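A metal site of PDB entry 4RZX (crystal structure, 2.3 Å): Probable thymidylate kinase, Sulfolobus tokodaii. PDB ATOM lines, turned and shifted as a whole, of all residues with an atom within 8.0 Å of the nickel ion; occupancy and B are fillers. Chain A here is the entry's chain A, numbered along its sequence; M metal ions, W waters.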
ATOM      1  N   TRP A  39     -18.401   8.031   5.425  1.00  0.00           N
ATOM      2  CA  TRP A  39     -17.469   8.731   4.557  1.00  0.00           C
ATOM      3  C   TRP A  39     -17.700   8.558   3.046  1.00  0.00           C
ATOM      4  O   TRP A  39     -17.737   9.545   2.276  1.00  0.00           O
ATOM      5  CB  TRP A  39     -16.063   8.237   4.789  1.00  0.00           C
ATOM      6  CG  TRP A  39     -15.030   9.012   3.999  1.00  0.00           C
ATOM      7  CD1 TRP A  39     -14.388   8.625   2.857  1.00  0.00           C
ATOM      8  CD2 TRP A  39     -14.515  10.273   4.353  1.00  0.00           C
ATOM      9  NE1 TRP A  39     -13.523   9.593   2.459  1.00  0.00           N
ATOM     10  CE2 TRP A  39     -13.562  10.622   3.367  1.00  0.00           C
ATOM     11  CE3 TRP A  39     -14.768  11.164   5.400  1.00  0.00           C
ATOM     12  CZ2 TRP A  39     -12.886  11.839   3.378  1.00  0.00           C
ATOM     13  CZ3 TRP A  39     -14.066  12.397   5.431  1.00  0.00           C
ATOM     14  CH2 TRP A  39     -13.155  12.718   4.436  1.00  0.00           C
ATOM     15  N   ASN A  40     -17.809   7.301   2.633  1.00  0.00           N
ATOM     16  CA  ASN A  40     -18.025   6.938   1.226  1.00  0.00           C
ATOM     17  C   ASN A  40     -19.322   7.424   0.566  1.00  0.00           C
ATOM     18  O   ASN A  40     -19.443   7.231  -0.621  1.00  0.00           O
ATOM     19  CB  ASN A  40     -17.962   5.404   1.067  1.00  0.00           C
ATOM     20  CG  ASN A  40     -16.557   4.886   1.180  1.00  0.00           C
ATOM     21  OD1 ASN A  40     -15.584   5.662   1.185  1.00  0.00           O
ATOM     22  ND2 ASN A  40     -16.430   3.579   1.339  1.00  0.00           N
ATOM     23  N   SER A  42     -20.761  10.139  -0.761  1.00  0.00           N
ATOM     24  CA  SER A  42     -20.471  11.458  -1.288  1.00  0.00           C
ATOM     25  C   SER A  42     -21.768  12.144  -1.713  1.00  0.00           C
ATOM     26  O   SER A  42     -22.764  11.491  -2.004  1.00  0.00           O
ATOM     27  CB  SER A  42     -19.530  11.274  -2.480  1.00  0.00           C
ATOM     28  OG  SER A  42     -18.396  10.481  -2.102  1.00  0.00           O
ATOM     29  N   HIS A  46     -19.468  16.410  -5.308  1.00  0.00           N
ATOM     30  CA  HIS A  46     -18.725  15.284  -5.828  1.00  0.00           C
ATOM     31  C   HIS A  46     -19.340  14.733  -7.117  1.00  0.00           C
ATOM     32  O   HIS A  46     -18.651  14.518  -8.115  1.00  0.00           O
ATOM     33  CB  HIS A  46     -18.652  14.211  -4.727  1.00  0.00           C
ATOM     34  CG  HIS A  46     -18.261  12.838  -5.192  1.00  0.00           C
ATOM     35  ND1 HIS A  46     -19.130  12.021  -5.887  1.00  0.00           N
ATOM     36  CD2 HIS A  46     -17.153  12.093  -4.940  1.00  0.00           C
ATOM     37  CE1 HIS A  46     -18.545  10.857  -6.118  1.00  0.00           C
ATOM     38  NE2 HIS A  46     -17.368  10.865  -5.525  1.00  0.00           N
ATOM     39  N   ASP A  47     -20.637  14.477  -7.094  1.00  0.00           N
ATOM     40  CA  ASP A  47     -21.272  13.839  -8.253  1.00  0.00           C
ATOM     41  C   ASP A  47     -21.199  14.756  -9.428  1.00  0.00           C
ATOM     42  O   ASP A  47     -20.944  14.299 -10.516  1.00  0.00           O
ATOM     43  CB  ASP A  47     -22.743  13.393  -7.973  1.00  0.00           C
ATOM     44  CG  ASP A  47     -22.806  12.291  -6.880  1.00  0.00           C
ATOM     45  OD1 ASP A  47     -21.726  11.875  -6.342  1.00  0.00           O
ATOM     46  OD2 ASP A  47     -23.927  11.881  -6.528  1.00  0.00           O
ATOM     47  N   LYS A  50     -17.345  14.731 -10.771  1.00  0.00           N
ATOM     48  CA  LYS A  50     -17.035  13.481 -11.405  1.00  0.00           C
ATOM     49  C   LYS A  50     -17.778  13.284 -12.702  1.00  0.00           C
ATOM     50  O   LYS A  50     -17.136  12.972 -13.695  1.00  0.00           O
ATOM     51  CB  LYS A  50     -17.228  12.332 -10.441  1.00  0.00           C
ATOM     52  CG  LYS A  50     -16.157  12.323  -9.332  1.00  0.00           C
ATOM     53  CD  LYS A  50     -15.949  10.910  -8.822  1.00  0.00           C
ATOM     54  CE  LYS A  50     -14.985  10.770  -7.645  1.00  0.00           C
ATOM     55  NZ  LYS A  50     -14.975   9.348  -7.207  1.00  0.00           N
ATOM     56  N   PHE A  63      -8.468  14.161  -7.742  1.00  0.00           N
ATOM     57  CA  PHE A  63      -9.336  13.158  -7.091  1.00  0.00           C
ATOM     58  C   PHE A  63      -9.446  13.487  -5.600  1.00  0.00           C
ATOM     59  O   PHE A  63     -10.535  13.587  -5.043  1.00  0.00           O
ATOM     60  CB  PHE A  63      -8.703  11.779  -7.261  1.00  0.00           C
ATOM     61  CG  PHE A  63      -9.577  10.628  -6.845  1.00  0.00           C
ATOM     62  CD1 PHE A  63     -10.520  10.106  -7.714  1.00  0.00           C
ATOM     63  CD2 PHE A  63      -9.401  10.023  -5.616  1.00  0.00           C
ATOM     64  CE1 PHE A  63     -11.308   9.019  -7.344  1.00  0.00           C
ATOM     65  CE2 PHE A  63     -10.181   8.956  -5.250  1.00  0.00           C
ATOM     66  CZ  PHE A  63     -11.124   8.450  -6.111  1.00  0.00           C
ATOM     67  N   ILE A  66     -11.476  16.630  -4.831  1.00  0.00           N
ATOM     68  CA  ILE A  66     -12.900  16.520  -5.121  1.00  0.00           C
ATOM     69  C   ILE A  66     -13.553  15.994  -3.848  1.00  0.00           C
ATOM     70  O   ILE A  66     -14.513  16.549  -3.323  1.00  0.00           O
ATOM     71  CB  ILE A  66     -13.109  15.582  -6.302  1.00  0.00           C
ATOM     72  CG1 ILE A  66     -12.738  16.335  -7.584  1.00  0.00           C
ATOM     73  CG2 ILE A  66     -14.547  15.141  -6.410  1.00  0.00           C
ATOM     74  CD1 ILE A  66     -12.659  15.416  -8.788  1.00  0.00           C
ATOM     75  N   HIS A  67     -12.937  14.972  -3.273  1.00  0.00           N
ATOM     76  CA  HIS A  67     -13.465  14.389  -2.055  1.00  0.00           C
ATOM     77  C   HIS A  67     -13.387  15.271  -0.805  1.00  0.00           C
ATOM     78  O   HIS A  67     -14.351  15.311  -0.006  1.00  0.00           O
ATOM     79  CB  HIS A  67     -12.846  13.044  -1.853  1.00  0.00           C
ATOM     80  CG  HIS A  67     -13.263  12.078  -2.918  1.00  0.00           C
ATOM     81  ND1 HIS A  67     -12.565  11.914  -4.090  1.00  0.00           N
ATOM     82  CD2 HIS A  67     -14.330  11.237  -2.991  1.00  0.00           C
ATOM     83  CE1 HIS A  67     -13.161  11.010  -4.839  1.00  0.00           C
ATOM     84  NE2 HIS A  67     -14.221  10.558  -4.182  1.00  0.00           N
ATOM     85  N   ASP A  70     -16.224  17.976  -1.298  1.00  0.00           N
ATOM     86  CA  ASP A  70     -17.496  17.390  -0.935  1.00  0.00           C
ATOM     87  C   ASP A  70     -17.565  17.143   0.550  1.00  0.00           C
ATOM     88  O   ASP A  70     -18.567  17.484   1.178  1.00  0.00           O
ATOM     89  CB  ASP A  70     -17.698  16.084  -1.718  1.00  0.00           C
ATOM     90  CG  ASP A  70     -19.109  15.500  -1.566  1.00  0.00           C
ATOM     91  OD1 ASP A  70     -20.033  15.932  -2.328  1.00  0.00           O
ATOM     92  OD2 ASP A  70     -19.260  14.547  -0.762  1.00  0.00           O
ATOM     93  N   ARG A 101      -6.208   6.570   1.300  1.00  0.00           N
ATOM     94  CA  ARG A 101      -6.538   6.588  -0.160  1.00  0.00           C
ATOM     95  C   ARG A 101      -5.662   7.487  -1.026  1.00  0.00           C
ATOM     96  O   ARG A 101      -5.265   7.094  -2.142  1.00  0.00           O
ATOM     97  CB  ARG A 101      -8.014   6.977  -0.429  1.00  0.00           C
ATOM     98  CG  ARG A 101      -8.933   5.758  -0.498  1.00  0.00           C
ATOM     99  CD  ARG A 101     -10.429   5.985  -0.786  1.00  0.00           C
ATOM    100  NE  ARG A 101     -11.186   4.991   0.010  1.00  0.00           N
ATOM    101  CZ  ARG A 101     -12.525   4.851   0.127  1.00  0.00           C
ATOM    102  NH1 ARG A 101     -13.371   5.692  -0.487  1.00  0.00           N
ATOM    103  NH2 ARG A 101     -13.016   3.856   0.901  1.00  0.00           N
HETATM  104 NI    NI M   1     -15.659   9.460  -5.230  1.00  0.00          NI
HETATM  105  O   HOH W   1     -16.289   9.046  -3.576  1.00  0.00           O
HETATM  106  O   HOH W   2     -14.325   7.640  -5.206  1.00  0.00           O
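The nickel ion is bound by water W1 (1.8 Å), NE2 of His 67 (2.1 Å), NZ of Lys 50 (2.1 Å), NE2 of His 46 (2.2 Å) and water W2 (2.3 Å). The nickel ion has five donor atoms within binding distance.
A ring nitrogen (ND1) of His 67 is in hydrogen-bond range of the backbone carbonyl oxygen of Phe 63 (2.8 Å). The backbone NH of His 46 sits at hydrogen-bond distance from the side-chain carboxylate of Asp 70, at 3.1 Å. A ring nitrogen (ND1) of His 46 sits at hydrogen-bond distance from the side-chain carboxylate of Asp 47.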
